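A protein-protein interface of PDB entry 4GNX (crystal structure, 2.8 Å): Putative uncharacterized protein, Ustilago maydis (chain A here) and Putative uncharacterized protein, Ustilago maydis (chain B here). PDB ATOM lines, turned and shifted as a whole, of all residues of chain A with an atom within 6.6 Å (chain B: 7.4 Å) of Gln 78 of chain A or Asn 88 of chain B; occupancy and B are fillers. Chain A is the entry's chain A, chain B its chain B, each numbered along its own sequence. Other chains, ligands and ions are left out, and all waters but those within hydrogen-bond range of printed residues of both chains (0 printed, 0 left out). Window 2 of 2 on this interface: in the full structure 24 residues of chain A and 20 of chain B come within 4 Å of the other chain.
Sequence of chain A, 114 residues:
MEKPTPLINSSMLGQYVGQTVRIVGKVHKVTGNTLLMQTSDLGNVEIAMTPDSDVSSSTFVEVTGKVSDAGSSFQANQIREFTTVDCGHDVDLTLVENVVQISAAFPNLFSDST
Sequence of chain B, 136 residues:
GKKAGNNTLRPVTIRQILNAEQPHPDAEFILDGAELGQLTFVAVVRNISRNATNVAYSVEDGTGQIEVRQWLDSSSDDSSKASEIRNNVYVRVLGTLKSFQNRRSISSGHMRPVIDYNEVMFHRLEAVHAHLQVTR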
ATOM      1  N   MET A  49       2.424   5.779   8.323  1.00  0.00           N
ATOM      2  CA  MET A  49       2.034   4.510   8.890  1.00  0.00           C
ATOM      3  C   MET A  49       0.528   4.234   8.772  1.00  0.00           C
ATOM      4  O   MET A  49      -0.298   5.152   8.856  1.00  0.00           O
ATOM      5  CB  MET A  49       2.482   4.493  10.353  1.00  0.00           C
ATOM      6  CG  MET A  49       2.967   3.149  10.880  1.00  0.00           C
ATOM      7  SD  MET A  49       4.275   2.338   9.931  1.00  0.00           S
ATOM      8  CE  MET A  49       5.381   3.729   9.686  1.00  0.00           C
ATOM      9  N   THR A  50       0.198   2.959   8.562  1.00  0.00           N
ATOM     10  CA  THR A  50      -1.167   2.432   8.654  1.00  0.00           C
ATOM     11  C   THR A  50      -1.776   2.725  10.037  1.00  0.00           C
ATOM     12  O   THR A  50      -1.067   2.716  11.046  1.00  0.00           O
ATOM     13  CB  THR A  50      -1.164   0.905   8.354  1.00  0.00           C
ATOM     14  OG1 THR A  50      -0.999   0.707   6.955  1.00  0.00           O
ATOM     15  CG2 THR A  50      -2.452   0.216   8.746  1.00  0.00           C
ATOM     16  N   GLU A  62      11.096  -3.458   9.871  1.00  0.00           N
ATOM     17  CA  GLU A  62      11.214  -3.625   8.404  1.00  0.00           C
ATOM     18  C   GLU A  62       9.927  -3.208   7.737  1.00  0.00           C
ATOM     19  O   GLU A  62       8.879  -3.812   7.967  1.00  0.00           O
ATOM     20  CB  GLU A  62      11.573  -5.061   7.978  1.00  0.00           C
ATOM     21  CG  GLU A  62      11.846  -5.192   6.480  1.00  0.00           C
ATOM     22  CD  GLU A  62      11.910  -6.639   5.987  1.00  0.00           C
ATOM     23  OE1 GLU A  62      10.848  -7.213   5.631  1.00  0.00           O
ATOM     24  OE2 GLU A  62      13.026  -7.223   5.925  1.00  0.00           O
ATOM     25  N   VAL A  63      10.009  -2.179   6.900  1.00  0.00           N
ATOM     26  CA  VAL A  63       8.799  -1.673   6.234  1.00  0.00           C
ATOM     27  C   VAL A  63       8.764  -2.072   4.787  1.00  0.00           C
ATOM     28  O   VAL A  63       9.761  -1.895   4.082  1.00  0.00           O
ATOM     29  CB  VAL A  63       8.725  -0.145   6.248  1.00  0.00           C
ATOM     30  CG1 VAL A  63       7.518   0.307   5.444  1.00  0.00           C
ATOM     31  CG2 VAL A  63       8.699   0.360   7.677  1.00  0.00           C
ATOM     32  N   THR A  64       7.636  -2.613   4.351  1.00  0.00           N
ATOM     33  CA  THR A  64       7.392  -2.715   2.929  1.00  0.00           C
ATOM     34  C   THR A  64       6.500  -1.536   2.607  1.00  0.00           C
ATOM     35  O   THR A  64       5.422  -1.374   3.195  1.00  0.00           O
ATOM     36  CB  THR A  64       6.755  -4.058   2.496  1.00  0.00           C
ATOM     37  OG1 THR A  64       7.601  -5.152   2.873  1.00  0.00           O
ATOM     38  CG2 THR A  64       6.612  -4.116   1.008  1.00  0.00           C
ATOM     39  N   GLY A  65       6.960  -0.688   1.699  1.00  0.00           N
ATOM     40  CA  GLY A  65       6.210   0.515   1.391  1.00  0.00           C
ATOM     41  C   GLY A  65       6.462   1.045   0.013  1.00  0.00           C
ATOM     42  O   GLY A  65       7.371   0.594  -0.682  1.00  0.00           O
ATOM     43  N   GLN A  75       4.626   5.478   1.845  1.00  0.00           N
ATOM     44  CA  GLN A  75       3.325   4.963   2.267  1.00  0.00           C
ATOM     45  C   GLN A  75       3.500   3.505   2.675  1.00  0.00           C
ATOM     46  O   GLN A  75       3.620   2.648   1.811  1.00  0.00           O
ATOM     47  CB  GLN A  75       2.231   5.166   1.179  1.00  0.00           C
ATOM     48  CG  GLN A  75       0.786   4.815   1.584  1.00  0.00           C
ATOM     49  CD  GLN A  75      -0.325   5.634   0.877  1.00  0.00           C
ATOM     50  OE1 GLN A  75      -0.116   6.230  -0.194  1.00  0.00           O
ATOM     51  NE2 GLN A  75      -1.526   5.660   1.487  1.00  0.00           N
ATOM     52  N   ALA A  76       3.525   3.238   3.987  1.00  0.00           N
ATOM     53  CA  ALA A  76       3.670   1.872   4.496  1.00  0.00           C
ATOM     54  C   ALA A  76       2.532   0.973   4.043  1.00  0.00           C
ATOM     55  O   ALA A  76       1.375   1.325   4.199  1.00  0.00           O
ATOM     56  CB  ALA A  76       3.782   1.856   6.024  1.00  0.00           C
ATOM     57  N   ASN A  77       2.883  -0.182   3.478  1.00  0.00           N
ATOM     58  CA  ASN A  77       1.922  -1.234   3.170  1.00  0.00           C
ATOM     59  C   ASN A  77       1.909  -2.204   4.357  1.00  0.00           C
ATOM     60  O   ASN A  77       0.885  -2.375   5.019  1.00  0.00           O
ATOM     61  CB  ASN A  77       2.250  -1.932   1.830  1.00  0.00           C
ATOM     62  CG  ASN A  77       1.974  -1.043   0.583  1.00  0.00           C
ATOM     63  OD1 ASN A  77       1.073  -0.186   0.576  1.00  0.00           O
ATOM     64  ND2 ASN A  77       2.735  -1.273  -0.491  1.00  0.00           N
ATOM     65  N   GLN A  78       3.069  -2.799   4.651  1.00  0.00           N
ATOM     66  CA  GLN A  78       3.216  -3.751   5.760  1.00  0.00           C
ATOM     67  C   GLN A  78       4.402  -3.425   6.628  1.00  0.00           C
ATOM     68  O   GLN A  78       5.265  -2.660   6.247  1.00  0.00           O
ATOM     69  CB  GLN A  78       3.325  -5.197   5.272  1.00  0.00           C
ATOM     70  CG  GLN A  78       1.980  -5.899   5.118  1.00  0.00           C
ATOM     71  CD  GLN A  78       1.242  -6.194   6.444  1.00  0.00           C
ATOM     72  OE1 GLN A  78       0.562  -7.232   6.575  1.00  0.00           O
ATOM     73  NE2 GLN A  78       1.348  -5.276   7.424  1.00  0.00           N
ATOM     74  N   ILE A  79       4.442  -3.996   7.818  1.00  0.00           N
ATOM     75  CA  ILE A  79       5.523  -3.683   8.743  1.00  0.00           C
ATOM     76  C   ILE A  79       5.900  -4.905   9.615  1.00  0.00           C
ATOM     77  O   ILE A  79       5.021  -5.595  10.149  1.00  0.00           O
ATOM     78  CB  ILE A  79       5.190  -2.437   9.622  1.00  0.00           C
ATOM     79  CG1 ILE A  79       4.853  -1.172   8.785  1.00  0.00           C
ATOM     80  CG2 ILE A  79       6.343  -2.143  10.561  1.00  0.00           C
ATOM     81  CD1 ILE A  79       3.366  -0.860   8.582  1.00  0.00           C
ATOM     82  N   ARG A  80       7.210  -5.134   9.754  1.00  0.00           N
ATOM     83  CA  ARG A  80       7.798  -6.249  10.502  1.00  0.00           C
ATOM     84  C   ARG A  80       8.654  -5.820  11.724  1.00  0.00           C
ATOM     85  O   ARG A  80       9.546  -4.997  11.590  1.00  0.00           O
ATOM     86  CB  ARG A  80       8.682  -7.041   9.542  1.00  0.00           C
ATOM     87  CG  ARG A  80       8.417  -8.533   9.501  1.00  0.00           C
ATOM     88  CD  ARG A  80       8.297  -9.176  10.891  1.00  0.00           C
ATOM     89  NE  ARG A  80       7.108  -8.726  11.650  1.00  0.00           N
ATOM     90  CZ  ARG A  80       6.468  -9.413  12.603  1.00  0.00           C
ATOM     91  NH1 ARG A  80       6.849 -10.640  12.965  1.00  0.00           N
ATOM     92  NH2 ARG A  80       5.414  -8.859  13.189  1.00  0.00           N
ATOM     93  N   GLU A  81       8.420  -6.396  12.898  1.00  0.00           N
ATOM     94  CA  GLU A  81       9.219  -6.093  14.095  1.00  0.00           C
ATOM     95  C   GLU A  81      10.562  -6.856  14.149  1.00  0.00           C
ATOM     96  O   GLU A  81      10.734  -7.817  13.407  1.00  0.00           O
ATOM     97  CB  GLU A  81       8.388  -6.434  15.329  1.00  0.00           C
ATOM     98  CG  GLU A  81       8.581  -5.492  16.504  1.00  0.00           C
ATOM     99  CD  GLU A  81       9.962  -5.626  17.097  1.00  0.00           C
ATOM    100  OE1 GLU A  81      10.250  -6.689  17.697  1.00  0.00           O
ATOM    101  OE2 GLU A  81      10.769  -4.681  16.933  1.00  0.00           O
ATOM    102  N   ALA B  43      11.946 -16.343   4.587  1.00  0.00           N
ATOM    103  CA  ALA B  43      10.880 -15.656   3.864  1.00  0.00           C
ATOM    104  C   ALA B  43       9.792 -15.258   4.839  1.00  0.00           C
ATOM    105  O   ALA B  43       9.812 -15.684   6.005  1.00  0.00           O
ATOM    106  CB  ALA B  43      10.300 -16.559   2.797  1.00  0.00           C
ATOM    107  N   VAL B  44       8.844 -14.455   4.342  1.00  0.00           N
ATOM    108  CA  VAL B  44       7.716 -13.992   5.134  1.00  0.00           C
ATOM    109  C   VAL B  44       6.421 -14.660   4.683  1.00  0.00           C
ATOM    110  O   VAL B  44       6.104 -14.705   3.480  1.00  0.00           O
ATOM    111  CB  VAL B  44       7.570 -12.471   5.062  1.00  0.00           C
ATOM    112  CG1 VAL B  44       6.435 -11.985   5.962  1.00  0.00           C
ATOM    113  CG2 VAL B  44       8.864 -11.827   5.495  1.00  0.00           C
ATOM    114  N   VAL B  45       5.692 -15.201   5.658  1.00  0.00           N
ATOM    115  CA  VAL B  45       4.435 -15.842   5.419  1.00  0.00           C
ATOM    116  C   VAL B  45       3.445 -14.742   5.110  1.00  0.00           C
ATOM    117  O   VAL B  45       3.330 -13.765   5.856  1.00  0.00           O
ATOM    118  CB  VAL B  45       3.972 -16.578   6.677  1.00  0.00           C
ATOM    119  CG1 VAL B  45       2.739 -17.431   6.380  1.00  0.00           C
ATOM    120  CG2 VAL B  45       5.100 -17.413   7.242  1.00  0.00           C
ATOM    121  N   ARG B  46       2.719 -14.909   4.021  1.00  0.00           N
ATOM    122  CA  ARG B  46       1.744 -13.925   3.604  1.00  0.00           C
ATOM    123  C   ARG B  46       0.317 -14.454   3.605  1.00  0.00           C
ATOM    124  O   ARG B  46      -0.630 -13.679   3.757  1.00  0.00           O
ATOM    125  CB  ARG B  46       2.088 -13.411   2.221  1.00  0.00           C
ATOM    126  CG  ARG B  46       3.289 -12.506   2.215  1.00  0.00           C
ATOM    127  CD  ARG B  46       3.104 -11.234   3.028  1.00  0.00           C
ATOM    128  NE  ARG B  46       4.288 -10.391   2.893  1.00  0.00           N
ATOM    129  CZ  ARG B  46       4.632  -9.420   3.728  1.00  0.00           C
ATOM    130  NH1 ARG B  46       3.877  -9.138   4.794  1.00  0.00           N
ATOM    131  NH2 ARG B  46       5.741  -8.729   3.488  1.00  0.00           N
ATOM    132  N   ASN B  47       0.173 -15.764   3.395  1.00  0.00           N
ATOM    133  CA  ASN B  47      -1.112 -16.461   3.527  1.00  0.00           C
ATOM    134  C   ASN B  47      -0.971 -17.913   4.055  1.00  0.00           C
ATOM    135  O   ASN B  47       0.073 -18.561   3.860  1.00  0.00           O
ATOM    136  CB  ASN B  47      -1.886 -16.414   2.210  1.00  0.00           C
ATOM    137  CG  ASN B  47      -3.193 -17.180   2.274  1.00  0.00           C
ATOM    138  OD1 ASN B  47      -3.345 -18.216   1.620  1.00  0.00           O
ATOM    139  ND2 ASN B  47      -4.134 -16.690   3.082  1.00  0.00           N
ATOM    140  N   ILE B  48      -2.003 -18.394   4.749  1.00  0.00           N
ATOM    141  CA  ILE B  48      -1.994 -19.734   5.307  1.00  0.00           C
ATOM    142  C   ILE B  48      -3.313 -20.423   5.008  1.00  0.00           C
ATOM    143  O   ILE B  48      -4.364 -20.019   5.487  1.00  0.00           O
ATOM    144  CB  ILE B  48      -1.760 -19.746   6.837  1.00  0.00           C
ATOM    145  CG1 ILE B  48      -0.490 -18.992   7.221  1.00  0.00           C
ATOM    146  CG2 ILE B  48      -1.674 -21.176   7.342  1.00  0.00           C
ATOM    147  CD1 ILE B  48      -0.328 -18.763   8.710  1.00  0.00           C
ATOM    148  N   SER B  58       1.753 -19.177   1.727  1.00  0.00           N
ATOM    149  CA  SER B  58       2.243 -18.373   0.629  1.00  0.00           C
ATOM    150  C   SER B  58       3.389 -17.610   1.195  1.00  0.00           C
ATOM    151  O   SER B  58       3.292 -17.006   2.250  1.00  0.00           O
ATOM    152  CB  SER B  58       1.202 -17.413   0.114  1.00  0.00           C
ATOM    153  OG  SER B  58       1.792 -16.596  -0.873  1.00  0.00           O
ATOM    154  N   GLU B  60       7.135 -15.300   0.667  1.00  0.00           N
ATOM    155  CA  GLU B  60       7.718 -14.232  -0.128  1.00  0.00           C
ATOM    156  C   GLU B  60       8.939 -13.626   0.604  1.00  0.00           C
ATOM    157  O   GLU B  60       8.863 -13.358   1.817  1.00  0.00           O
ATOM    158  CB  GLU B  60       6.611 -13.198  -0.415  1.00  0.00           C
ATOM    159  CG  GLU B  60       7.093 -11.868  -0.949  1.00  0.00           C
ATOM    160  CD  GLU B  60       7.406 -10.887   0.164  1.00  0.00           C
ATOM    161  OE1 GLU B  60       6.536 -10.730   1.064  1.00  0.00           O
ATOM    162  OE2 GLU B  60       8.504 -10.270   0.142  1.00  0.00           O
ATOM    163  N   ARG B  86       2.462 -17.338  11.946  1.00  0.00           N
ATOM    164  CA  ARG B  86       1.356 -16.513  11.503  1.00  0.00           C
ATOM    165  C   ARG B  86       1.778 -15.636  10.336  1.00  0.00           C
ATOM    166  O   ARG B  86       2.946 -15.603   9.966  1.00  0.00           O
ATOM    167  CB  ARG B  86       0.849 -15.679  12.666  1.00  0.00           C
ATOM    168  CG  ARG B  86      -0.082 -16.486  13.551  1.00  0.00           C
ATOM    169  CD  ARG B  86       0.224 -16.302  15.023  1.00  0.00           C
ATOM    170  NE  ARG B  86      -0.653 -15.308  15.644  1.00  0.00           N
ATOM    171  CZ  ARG B  86      -0.348 -14.017  15.789  1.00  0.00           C
ATOM    172  NH1 ARG B  86       0.836 -13.540  15.353  1.00  0.00           N
ATOM    173  NH2 ARG B  86      -1.231 -13.207  16.380  1.00  0.00           N
ATOM    174  N   ASN B  87       0.818 -14.950   9.735  1.00  0.00           N
ATOM    175  CA  ASN B  87       1.100 -14.050   8.634  1.00  0.00           C
ATOM    176  C   ASN B  87       2.075 -12.950   9.013  1.00  0.00           C
ATOM    177  O   ASN B  87       2.143 -12.543  10.173  1.00  0.00           O
ATOM    178  CB  ASN B  87      -0.195 -13.445   8.120  1.00  0.00           C
ATOM    179  CG  ASN B  87      -0.854 -14.328   7.115  1.00  0.00           C
ATOM    180  OD1 ASN B  87      -0.218 -15.246   6.593  1.00  0.00           O
ATOM    181  ND2 ASN B  87      -2.113 -14.076   6.827  1.00  0.00           N
ATOM    182  N   ASN B  88       2.836 -12.481   8.034  1.00  0.00           N
ATOM    183  CA  ASN B  88       3.698 -11.337   8.241  1.00  0.00           C
ATOM    184  C   ASN B  88       4.847 -11.617   9.239  1.00  0.00           C
ATOM    185  O   ASN B  88       5.262 -10.745  10.011  1.00  0.00           O
ATOM    186  CB  ASN B  88       2.854 -10.124   8.631  1.00  0.00           C
ATOM    187  CG  ASN B  88       3.605  -8.820   8.494  1.00  0.00           C
ATOM    188  OD1 ASN B  88       4.384  -8.610   7.541  1.00  0.00           O
ATOM    189  ND2 ASN B  88       3.374  -7.922   9.454  1.00  0.00           N
ATOM    190  N   VAL B  89       5.377 -12.839   9.164  1.00  0.00           N
ATOM    191  CA  VAL B  89       6.392 -13.357  10.096  1.00  0.00           C
ATOM    192  C   VAL B  89       7.537 -14.010   9.304  1.00  0.00           C
ATOM    193  O   VAL B  89       7.296 -14.785   8.376  1.00  0.00           O
ATOM    194  CB  VAL B  89       5.749 -14.395  11.077  1.00  0.00           C
ATOM    195  CG1 VAL B  89       6.775 -15.381  11.600  1.00  0.00           C
ATOM    196  CG2 VAL B  89       5.023 -13.713  12.231  1.00  0.00           C
ATOM    197  N   TYR B  90       8.780 -13.709   9.657  1.00  0.00           N
ATOM    198  CA  TYR B  90       9.886 -14.399   9.008  1.00  0.00           C
ATOM    199  C   TYR B  90      10.033 -15.849   9.460  1.00  0.00           C
ATOM    200  O   TYR B  90       9.793 -16.186  10.625  1.00  0.00           O
ATOM    201  CB  TYR B  90      11.186 -13.643   9.170  1.00  0.00           C
ATOM    202  CG  TYR B  90      11.401 -12.604   8.089  1.00  0.00           C
ATOM    203  CD1 TYR B  90      11.110 -11.273   8.320  1.00  0.00           C
ATOM    204  CD2 TYR B  90      11.908 -12.961   6.827  1.00  0.00           C
ATOM    205  CE1 TYR B  90      11.319 -10.325   7.342  1.00  0.00           C
ATOM    206  CE2 TYR B  90      12.124 -12.014   5.839  1.00  0.00           C
ATOM    207  CZ  TYR B  90      11.812 -10.702   6.097  1.00  0.00           C
ATOM    208  OH  TYR B  90      11.988  -9.736   5.135  1.00  0.00           O
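The side-chain carboxylate (OE1) of Glu 62 of chain A is in hydrogen-bond range of the side-chain hydroxyl (OH) of Tyr 90 of chain B (2.8 Å). The backbone carbonyl oxygen (O) of Ile 79 of chain A lies within hydrogen-bond range of the side-chain amide nitrogen (ND2) of Asn 88 of chain B (2.9 Å). NE of Arg 80 of chain A sits close to O of Asn 88 of chain B (3.2 Å).
The backbone NH of Glu 62 of chain A sits at hydrogen-bond distance from the backbone carbonyl oxygen of Arg 80 of chain A (2.8 Å). O of Val 45 of chain B lies within hydrogen-bond range of N of Asn 88 of chain B (2.6 Å). N of Val 45 of chain B lies within hydrogen-bond range of O of Val 89 of chain B. The side-chain carboxylate (OE1) of Glu 60 of chain B is in salt-bridge range of the guanidinium group (NE) of Arg 46 of chain B (2.9 Å). The side-chain amide oxygen of Asn 87 of chain B lies close to the backbone carbonyl oxygen of Arg 46 of chain B, 3.3 Å away. The guanidinium group (NH1) of Arg 46 of chain B sits at hydrogen-bond distance from the side-chain amide oxygen (OD1) of Asn 88 of chain B, 2.8 Å away.
Among the printed residues, merely in contact across the chains: Arg 80 of chain A with Val 89 of chain B, Gln 78 of chain A with Arg 46 of chain B and Gln 78 of chain A with Asn 88 of chain B.
Of the printed residues of chain B, Gln 78 of chain A touches Arg 46 and Asn 88. Asn 88 of chain B touches three residues of chain A. Of the printed residues of chain B, Arg 80 of chain A touches Asn 88 (3.2 Å) and Val 89 (3.6 Å). Of the printed residues of chain A, Val 89 of chain B touches Arg 80 (3.6 Å). Of the printed residues of chain B, Ile 79 of chain A touches Asn 88. Thr 50 of chain A touches none of the printed residues of chain B. Asn 77 of chain A touches none of the printed residues of chain B. The nearest residue of chain A that does not touch Asn 88 of chain B is Glu 81 of chain A (6.1 Å).
Of the 13 printed residues of chain B, 4 touch a printed residue of chain A. Printed residues of chain B that touch a printed residue of chain A: Arg 46, Asn 88, Val 89 and Tyr 90. Of the 13 printed residues of chain A, 4 touch a printed residue of chain B. Along chain A the printed residues that touch a printed residue of chain B span positions 62 to 80. Among the printed residues, no Asp or Glu carboxylate lies within 4 Å of a Lys or Arg side-chain nitrogen of the other chain.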
